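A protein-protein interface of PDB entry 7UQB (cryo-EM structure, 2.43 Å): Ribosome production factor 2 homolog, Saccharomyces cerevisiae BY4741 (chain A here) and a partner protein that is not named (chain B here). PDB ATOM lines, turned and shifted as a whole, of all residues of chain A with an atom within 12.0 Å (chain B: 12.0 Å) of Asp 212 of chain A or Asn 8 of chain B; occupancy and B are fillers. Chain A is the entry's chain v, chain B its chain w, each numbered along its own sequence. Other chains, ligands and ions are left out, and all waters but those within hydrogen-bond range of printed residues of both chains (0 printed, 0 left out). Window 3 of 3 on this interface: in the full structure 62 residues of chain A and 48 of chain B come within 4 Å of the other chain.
Among the printed residues, merely in contact across the chains: Ser 211 of chain A with Asn 8 of chain B (3.2 Å), Ser 211 of chain A with Leu 9 of chain B (3.8 Å), Ser 211 of chain A with Val 11 of chain B (3.7 Å), Asp 212 of chain A with Asn 8 of chain B (3.8 Å), Gln 213 of chain A with Leu 9 of chain B (3.7 Å), Gln 213 of chain A with Pro 10 of chain B (3.3 Å), Pro 219 of chain A with Val 11 of chain B (3.4 Å), Arg 220 of chain A with Leu 9 of chain B (3.4 Å), Arg 220 of chain A with Val 11 of chain B (3.8 Å), Arg 220 of chain A with Gln 59 of chain B (3.6 Å), Ile 221 of chain A with Arg 55 of chain B (3.1 Å) and Glu 222 of chain A with Leu 9 of chain B (3.8 Å).
Printed residues of chain B that touch a printed residue of chain A: Asn 8, Leu 9, Pro 10, Val 11, Arg 55 and Gln 59. Hydrophobic or aromatic side chains of chain B that line the printed part of chain A: Leu 9, Pro 10 and Val 11. Of the 15 printed residues of chain A, 7 touch a printed residue of chain B. Hydrophobic or aromatic side chains of chain A within 4 Å of the printed part of chain B: Ile 221. Among the printed residues, no Asp or Glu carboxylate lies within 4 Å of a Lys or Arg side-chain nitrogen of the other chain.
Printed residues of chain A within 4 Å of Asn 8 of chain B: Ser 211, Asp 212 and Gln 213. Lys 210 of chain A touches none of the printed residues of chain B. Printed residues of chain B within 4 Å of Ser 211 of chain A: Asn 8 (3.2 Å), Leu 9 (3.8 Å) and Val 11 (3.7 Å). Printed residues of chain B within 4 Å of Gln 213 of chain A: Asn 8, Leu 9 and Pro 10. No residue of chain B comes within 4 Å of Gly 214 of chain A. No residue of chain B comes within 4 Å of Gly 215 of chain A. Of chain A, only Ser 211, Gln 213, Arg 220 and Glu 222 come within 4 Å of Leu 9 of chain B. Pro 10 of chain B touches just these residues of chain A: Gln 213 (3.3 Å) and Arg 220 (2.3 Å). Printed residues of chain A within 4 Å of Arg 55 of chain B: Arg 220 (3.1 Å) and Ile 221 (3.1 Å). Of the printed residues of chain B, Pro 219 of chain A touches Val 11 (3.4 Å) and Gln 59 (3.4 Å). Of the printed residues of chain B, Glu 222 of chain A touches Leu 9 (3.8 Å). Printed residues of chain B within 4 Å of Arg 220 of chain A: Leu 9 (3.4 Å), Pro 10 (2.3 Å), Val 11 (3.8 Å), Arg 55 (3.1 Å) and Gln 59 (3.6 Å). Of the printed residues of chain A, Val 11 of chain B touches Ser 211, Pro 219 and Arg 220. Leu 218 of chain A touches none of the printed residues of chain B. Asn 63 of chain B touches none of the printed residues of chain A. The nearest residue of chain A that does not touch Asn 8 of chain B is Lys 210 of chain A (5.1 Å).
The side-chain amide nitrogen of Asn 63 of chain B is in hydrogen-bond range of the backbone carbonyl oxygen of Val 11 of chain B, 3.2 Å away. The side-chain hydroxyl (OG) of Ser 211 of chain A lies within hydrogen-bond range of the backbone NH (N) of Gly 214 of chain A (3.0 Å). The side-chain hydroxyl of Ser 211 of chain A lies close to the backbone NH of Gln 213 of chain A (3.4 Å). The backbone carbonyl oxygen (O) of Tyr 209 of chain A is in hydrogen-bond range of the backbone NH (N) of Arg 220 of chain A (2.7 Å). NH1 of Arg 55 of chain B lies within hydrogen-bond range of OE1 of Gln 59 of chain B, 2.9 Å away. NE of Arg 220 of chain A is in salt-bridge range of OE2 of Glu 222 of chain A.
NH1 of Arg 220 of chain A sits close to NH1 of Arg 55 of chain B (3.1 Å). N of Ile 221 of chain A lies within hydrogen-bond range of OE1 of Gln 59 of chain B (3.3 Å). O of Pro 219 of chain A lies within hydrogen-bond range of NE2 of Gln 59 of chain B, at 3.4 Å. The guanidinium group of Arg 220 of chain A lies close to the backbone carbonyl oxygen of Pro 10 of chain B. The side-chain amide nitrogen (NE2) of Gln 213 of chain A lies within hydrogen-bond range of the backbone carbonyl oxygen (O) of Asn 8 of chain B.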
ATOM      1  N   SER A 208      -5.343 -16.801  19.549  1.00  0.00           N
ATOM      2  CA  SER A 208      -5.822 -15.744  18.672  1.00  0.00           C
ATOM      3  C   SER A 208      -6.296 -14.565  19.509  1.00  0.00           C
ATOM      4  O   SER A 208      -7.059 -14.742  20.464  1.00  0.00           O
ATOM      5  CB  SER A 208      -6.948 -16.250  17.769  1.00  0.00           C
ATOM      6  OG  SER A 208      -7.999 -16.819  18.529  1.00  0.00           O
ATOM      7  N   TYR A 209      -5.833 -13.370  19.154  1.00  0.00           N
ATOM      8  CA  TYR A 209      -6.232 -12.141  19.819  1.00  0.00           C
ATOM      9  C   TYR A 209      -6.784 -11.171  18.787  1.00  0.00           C
ATOM     10  O   TYR A 209      -6.405 -11.210  17.613  1.00  0.00           O
ATOM     11  CB  TYR A 209      -5.064 -11.478  20.564  1.00  0.00           C
ATOM     12  CG  TYR A 209      -4.354 -12.369  21.556  1.00  0.00           C
ATOM     13  CD1 TYR A 209      -4.837 -12.529  22.848  1.00  0.00           C
ATOM     14  CD2 TYR A 209      -3.189 -13.039  21.204  1.00  0.00           C
ATOM     15  CE1 TYR A 209      -4.183 -13.341  23.759  1.00  0.00           C
ATOM     16  CE2 TYR A 209      -2.531 -13.849  22.107  1.00  0.00           C
ATOM     17  CZ  TYR A 209      -3.032 -13.997  23.382  1.00  0.00           C
ATOM     18  OH  TYR A 209      -2.374 -14.803  24.282  1.00  0.00           O
ATOM     19  N   LYS A 210      -7.687 -10.303  19.239  1.00  0.00           N
ATOM     20  CA  LYS A 210      -8.257  -9.281  18.371  1.00  0.00           C
ATOM     21  C   LYS A 210      -7.166  -8.334  17.885  1.00  0.00           C
ATOM     22  O   LYS A 210      -6.365  -7.831  18.679  1.00  0.00           O
ATOM     23  CB  LYS A 210      -9.342  -8.509  19.120  1.00  0.00           C
ATOM     24  CG  LYS A 210     -10.052  -7.461  18.290  1.00  0.00           C
ATOM     25  CD  LYS A 210     -10.999  -8.096  17.290  1.00  0.00           C
ATOM     26  CE  LYS A 210     -11.702  -7.033  16.465  1.00  0.00           C
ATOM     27  NZ  LYS A 210     -12.399  -6.038  17.325  1.00  0.00           N
ATOM     28  N   SER A 211      -7.140  -8.088  16.574  1.00  0.00           N
ATOM     29  CA  SER A 211      -6.034  -7.344  15.981  1.00  0.00           C
ATOM     30  C   SER A 211      -6.245  -5.838  16.038  1.00  0.00           C
ATOM     31  O   SER A 211      -5.265  -5.091  16.128  1.00  0.00           O
ATOM     32  CB  SER A 211      -5.826  -7.778  14.530  1.00  0.00           C
ATOM     33  OG  SER A 211      -6.851  -7.270  13.696  1.00  0.00           O
ATOM     34  N   ASP A 212      -7.497  -5.382  15.935  1.00  0.00           N
ATOM     35  CA  ASP A 212      -7.889  -3.972  15.966  1.00  0.00           C
ATOM     36  C   ASP A 212      -7.330  -3.181  14.783  1.00  0.00           C
ATOM     37  O   ASP A 212      -7.479  -1.956  14.723  1.00  0.00           O
ATOM     38  CB  ASP A 212      -7.472  -3.318  17.290  1.00  0.00           C
ATOM     39  CG  ASP A 212      -8.332  -2.123  17.647  1.00  0.00           C
ATOM     40  OD1 ASP A 212      -9.428  -1.986  17.062  1.00  0.00           O
ATOM     41  OD2 ASP A 212      -7.909  -1.318  18.501  1.00  0.00           O
ATOM     42  N   GLN A 213      -6.698  -3.866  13.835  1.00  0.00           N
ATOM     43  CA  GLN A 213      -6.232  -3.257  12.597  1.00  0.00           C
ATOM     44  C   GLN A 213      -6.742  -3.963  11.353  1.00  0.00           C
ATOM     45  O   GLN A 213      -6.984  -3.300  10.342  1.00  0.00           O
ATOM     46  CB  GLN A 213      -4.697  -3.225  12.554  1.00  0.00           C
ATOM     47  CG  GLN A 213      -4.071  -2.188  13.475  1.00  0.00           C
ATOM     48  CD  GLN A 213      -2.558  -2.159  13.383  1.00  0.00           C
ATOM     49  OE1 GLN A 213      -1.949  -2.995  12.715  1.00  0.00           O
ATOM     50  NE2 GLN A 213      -1.944  -1.193  14.056  1.00  0.00           N
ATOM     51  N   GLY A 214      -6.908  -5.281  11.399  1.00  0.00           N
ATOM     52  CA  GLY A 214      -7.508  -6.043  10.329  1.00  0.00           C
ATOM     53  C   GLY A 214      -8.976  -6.356  10.519  1.00  0.00           C
ATOM     54  O   GLY A 214      -9.514  -7.193   9.783  1.00  0.00           O
ATOM     55  N   GLY A 215      -9.642  -5.719  11.476  1.00  0.00           N
ATOM     56  CA  GLY A 215     -11.049  -5.947  11.702  1.00  0.00           C
ATOM     57  C   GLY A 215     -11.320  -7.173  12.554  1.00  0.00           C
ATOM     58  O   GLY A 215     -10.420  -7.818  13.098  1.00  0.00           O
ATOM     59  N   LYS A 216     -12.607  -7.490  12.666  1.00  0.00           N
ATOM     60  CA  LYS A 216     -13.051  -8.650  13.425  1.00  0.00           C
ATOM     61  C   LYS A 216     -12.967  -9.944  12.630  1.00  0.00           C
ATOM     62  O   LYS A 216     -13.257 -11.011  13.182  1.00  0.00           O
ATOM     63  CB  LYS A 216     -14.483  -8.431  13.923  1.00  0.00           C
ATOM     64  CG  LYS A 216     -15.434  -7.901  12.864  1.00  0.00           C
ATOM     65  CD  LYS A 216     -16.711  -7.363  13.491  1.00  0.00           C
ATOM     66  CE  LYS A 216     -17.502  -8.464  14.178  1.00  0.00           C
ATOM     67  NZ  LYS A 216     -17.992  -9.477  13.204  1.00  0.00           N
ATOM     68  N   ARG A 217     -12.580  -9.880  11.356  1.00  0.00           N
ATOM     69  CA  ARG A 217     -12.425 -11.073  10.537  1.00  0.00           C
ATOM     70  C   ARG A 217     -10.996 -11.600  10.505  1.00  0.00           C
ATOM     71  O   ARG A 217     -10.797 -12.780  10.199  1.00  0.00           O
ATOM     72  CB  ARG A 217     -12.888 -10.794   9.101  1.00  0.00           C
ATOM     73  CG  ARG A 217     -14.199 -10.023   9.008  1.00  0.00           C
ATOM     74  CD  ARG A 217     -15.358 -10.801   9.606  1.00  0.00           C
ATOM     75  NE  ARG A 217     -15.711 -11.962   8.801  1.00  0.00           N
ATOM     76  CZ  ARG A 217     -16.630 -11.958   7.845  1.00  0.00           C
ATOM     77  NH1 ARG A 217     -17.316 -10.866   7.549  1.00  0.00           N
ATOM     78  NH2 ARG A 217     -16.865 -13.079   7.167  1.00  0.00           N
ATOM     79  N   LEU A 218     -10.005 -10.764  10.807  1.00  0.00           N
ATOM     80  CA  LEU A 218      -8.597 -11.163  10.772  1.00  0.00           C
ATOM     81  C   LEU A 218      -7.957 -10.957  12.138  1.00  0.00           C
ATOM     82  O   LEU A 218      -7.571  -9.826  12.482  1.00  0.00           O
ATOM     83  CB  LEU A 218      -7.841 -10.374   9.706  1.00  0.00           C
ATOM     84  CG  LEU A 218      -8.423 -10.442   8.295  1.00  0.00           C
ATOM     85  CD1 LEU A 218      -7.564  -9.646   7.330  1.00  0.00           C
ATOM     86  CD2 LEU A 218      -8.558 -11.884   7.838  1.00  0.00           C
ATOM     87  N   PRO A 219      -7.819 -12.003  12.945  1.00  0.00           N
ATOM     88  CA  PRO A 219      -7.190 -11.856  14.260  1.00  0.00           C
ATOM     89  C   PRO A 219      -5.669 -11.905  14.175  1.00  0.00           C
ATOM     90  O   PRO A 219      -5.077 -12.177  13.130  1.00  0.00           O
ATOM     91  CB  PRO A 219      -7.734 -13.057  15.033  1.00  0.00           C
ATOM     92  CG  PRO A 219      -7.907 -14.099  13.982  1.00  0.00           C
ATOM     93  CD  PRO A 219      -8.343 -13.363  12.737  1.00  0.00           C
ATOM     94  N   ARG A 220      -5.045 -11.638  15.319  1.00  0.00           N
ATOM     95  CA  ARG A 220      -3.604 -11.745  15.492  1.00  0.00           C
ATOM     96  C   ARG A 220      -3.273 -13.084  16.139  1.00  0.00           C
ATOM     97  O   ARG A 220      -3.977 -13.537  17.045  1.00  0.00           O
ATOM     98  CB  ARG A 220      -3.078 -10.590  16.350  1.00  0.00           C
ATOM     99  CG  ARG A 220      -1.614 -10.686  16.755  1.00  0.00           C
ATOM    100  CD  ARG A 220      -0.670 -10.391  15.600  1.00  0.00           C
ATOM    101  NE  ARG A 220       0.705 -10.253  16.067  1.00  0.00           N
ATOM    102  CZ  ARG A 220       1.733  -9.909  15.302  1.00  0.00           C
ATOM    103  NH1 ARG A 220       1.583  -9.676  14.009  1.00  0.00           N
ATOM    104  NH2 ARG A 220       2.940  -9.798  15.847  1.00  0.00           N
ATOM    105  N   ILE A 221      -2.204 -13.716  15.667  1.00  0.00           N
ATOM    106  CA  ILE A 221      -1.809 -15.048  16.112  1.00  0.00           C
ATOM    107  C   ILE A 221      -0.612 -14.930  17.044  1.00  0.00           C
ATOM    108  O   ILE A 221       0.266 -14.084  16.839  1.00  0.00           O
ATOM    109  CB  ILE A 221      -1.494 -15.951  14.902  1.00  0.00           C
ATOM    110  CG1 ILE A 221      -2.714 -16.054  13.985  1.00  0.00           C
ATOM    111  CG2 ILE A 221      -1.059 -17.336  15.345  1.00  0.00           C
ATOM    112  CD1 ILE A 221      -3.938 -16.642  14.660  1.00  0.00           C
ATOM    113  N   GLU A 222      -0.595 -15.750  18.096  1.00  0.00           N
ATOM    114  CA  GLU A 222       0.569 -15.929  18.949  1.00  0.00           C
ATOM    115  C   GLU A 222       0.755 -17.417  19.214  1.00  0.00           C
ATOM    116  O   GLU A 222      -0.185 -18.206  19.109  1.00  0.00           O
ATOM    117  CB  GLU A 222       0.433 -15.168  20.274  1.00  0.00           C
ATOM    118  CG  GLU A 222       0.451 -13.657  20.123  1.00  0.00           C
ATOM    119  CD  GLU A 222       1.745 -13.147  19.522  1.00  0.00           C
ATOM    120  OE1 GLU A 222       2.815 -13.704  19.845  1.00  0.00           O
ATOM    121  OE2 GLU A 222       1.692 -12.188  18.722  1.00  0.00           O
ATOM    122  N   ASN B   8      -2.795  -3.911  19.638  1.00  0.00           N
ATOM    123  CA  ASN B   8      -3.093  -3.899  18.211  1.00  0.00           C
ATOM    124  C   ASN B   8      -1.839  -4.120  17.366  1.00  0.00           C
ATOM    125  O   ASN B   8      -1.311  -3.187  16.758  1.00  0.00           O
ATOM    126  CB  ASN B   8      -3.770  -2.583  17.815  1.00  0.00           C
ATOM    127  CG  ASN B   8      -2.870  -1.379  18.015  1.00  0.00           C
ATOM    128  OD1 ASN B   8      -1.654  -1.461  17.841  1.00  0.00           O
ATOM    129  ND2 ASN B   8      -3.466  -0.249  18.381  1.00  0.00           N
ATOM    130  N   LEU B   9      -1.366  -5.362  17.334  1.00  0.00           N
ATOM    131  CA  LEU B   9      -0.232  -5.702  16.495  1.00  0.00           C
ATOM    132  C   LEU B   9      -0.676  -5.832  15.037  1.00  0.00           C
ATOM    133  O   LEU B   9      -1.842  -6.127  14.760  1.00  0.00           O
ATOM    134  CB  LEU B   9       0.407  -7.004  16.968  1.00  0.00           C
ATOM    135  CG  LEU B   9       0.911  -7.008  18.411  1.00  0.00           C
ATOM    136  CD1 LEU B   9       1.563  -8.341  18.753  1.00  0.00           C
ATOM    137  CD2 LEU B   9       1.875  -5.858  18.643  1.00  0.00           C
ATOM    138  N   PRO B  10       0.227  -5.595  14.086  1.00  0.00           N
ATOM    139  CA  PRO B  10      -0.128  -5.785  12.674  1.00  0.00           C
ATOM    140  C   PRO B  10      -0.368  -7.250  12.346  1.00  0.00           C
ATOM    141  O   PRO B  10       0.155  -8.154  13.002  1.00  0.00           O
ATOM    142  CB  PRO B  10       1.095  -5.244  11.922  1.00  0.00           C
ATOM    143  CG  PRO B  10       1.808  -4.377  12.906  1.00  0.00           C
ATOM    144  CD  PRO B  10       1.567  -5.006  14.240  1.00  0.00           C
ATOM    145  N   VAL B  11      -1.178  -7.476  11.315  1.00  0.00           N
ATOM    146  CA  VAL B  11      -1.458  -8.817  10.820  1.00  0.00           C
ATOM    147  C   VAL B  11      -1.060  -8.964   9.352  1.00  0.00           C
ATOM    148  O   VAL B  11      -1.563  -9.839   8.659  1.00  0.00           O
ATOM    149  CB  VAL B  11      -2.937  -9.194  11.036  1.00  0.00           C
ATOM    150  CG1 VAL B  11      -3.213  -9.440  12.511  1.00  0.00           C
ATOM    151  CG2 VAL B  11      -3.846  -8.104  10.497  1.00  0.00           C
ATOM    152  N   THR B  12      -0.160  -8.111   8.874  1.00  0.00           N
ATOM    153  CA  THR B  12       0.318  -8.139   7.492  1.00  0.00           C
ATOM    154  C   THR B  12       1.804  -8.490   7.515  1.00  0.00           C
ATOM    155  O   THR B  12       2.664  -7.615   7.628  1.00  0.00           O
ATOM    156  CB  THR B  12       0.072  -6.803   6.793  1.00  0.00           C
ATOM    157  OG1 THR B  12       0.604  -5.737   7.589  1.00  0.00           O
ATOM    158  CG2 THR B  12      -1.417  -6.578   6.583  1.00  0.00           C
ATOM    159  N   VAL B  13       2.098  -9.781   7.398  1.00  0.00           N
ATOM    160  CA  VAL B  13       3.476 -10.260   7.396  1.00  0.00           C
ATOM    161  C   VAL B  13       4.114  -9.938   6.053  1.00  0.00           C
ATOM    162  O   VAL B  13       3.556 -10.253   4.994  1.00  0.00           O
ATOM    163  CB  VAL B  13       3.526 -11.769   7.688  1.00  0.00           C
ATOM    164  CG1 VAL B  13       4.939 -12.306   7.511  1.00  0.00           C
ATOM    165  CG2 VAL B  13       3.008 -12.058   9.089  1.00  0.00           C
ATOM    166  N   ARG B  55       5.646 -18.049  13.830  1.00  0.00           N
ATOM    167  CA  ARG B  55       4.565 -17.098  14.054  1.00  0.00           C
ATOM    168  C   ARG B  55       4.170 -16.406  12.757  1.00  0.00           C
ATOM    169  O   ARG B  55       2.984 -16.315  12.426  1.00  0.00           O
ATOM    170  CB  ARG B  55       5.000 -16.073  15.105  1.00  0.00           C
ATOM    171  CG  ARG B  55       3.901 -15.564  16.025  1.00  0.00           C
ATOM    172  CD  ARG B  55       2.934 -14.641  15.309  1.00  0.00           C
ATOM    173  NE  ARG B  55       3.610 -13.588  14.564  1.00  0.00           N
ATOM    174  CZ  ARG B  55       2.993 -12.712  13.783  1.00  0.00           C
ATOM    175  NH1 ARG B  55       1.680 -12.730  13.626  1.00  0.00           N
ATOM    176  NH2 ARG B  55       3.712 -11.796  13.141  1.00  0.00           N
ATOM    177  N   GLN B  59       0.714 -16.918  10.775  1.00  0.00           N
ATOM    178  CA  GLN B  59      -0.138 -15.763  10.508  1.00  0.00           C
ATOM    179  C   GLN B  59      -0.561 -15.722   9.046  1.00  0.00           C
ATOM    180  O   GLN B  59      -1.744 -15.514   8.738  1.00  0.00           O
ATOM    181  CB  GLN B  59       0.589 -14.474  10.894  1.00  0.00           C
ATOM    182  CG  GLN B  59      -0.215 -13.202  10.660  1.00  0.00           C
ATOM    183  CD  GLN B  59      -1.345 -13.029  11.656  1.00  0.00           C
ATOM    184  OE1 GLN B  59      -1.137 -12.549  12.770  1.00  0.00           O
ATOM    185  NE2 GLN B  59      -2.551 -13.415  11.258  1.00  0.00           N
ATOM    186  N   ASN B  63      -4.373 -16.371   7.707  1.00  0.00           N
ATOM    187  CA  ASN B  63      -5.005 -15.395   6.824  1.00  0.00           C
ATOM    188  C   ASN B  63      -5.573 -16.066   5.578  1.00  0.00           C
ATOM    189  O   ASN B  63      -6.710 -15.788   5.180  1.00  0.00           O
ATOM    190  CB  ASN B  63      -4.005 -14.305   6.436  1.00  0.00           C
ATOM    191  CG  ASN B  63      -3.811 -13.274   7.529  1.00  0.00           C
ATOM    192  OD1 ASN B  63      -4.076 -13.535   8.701  1.00  0.00           O
ATOM    193  ND2 ASN B  63      -3.349 -12.090   7.147  1.00  0.00           N
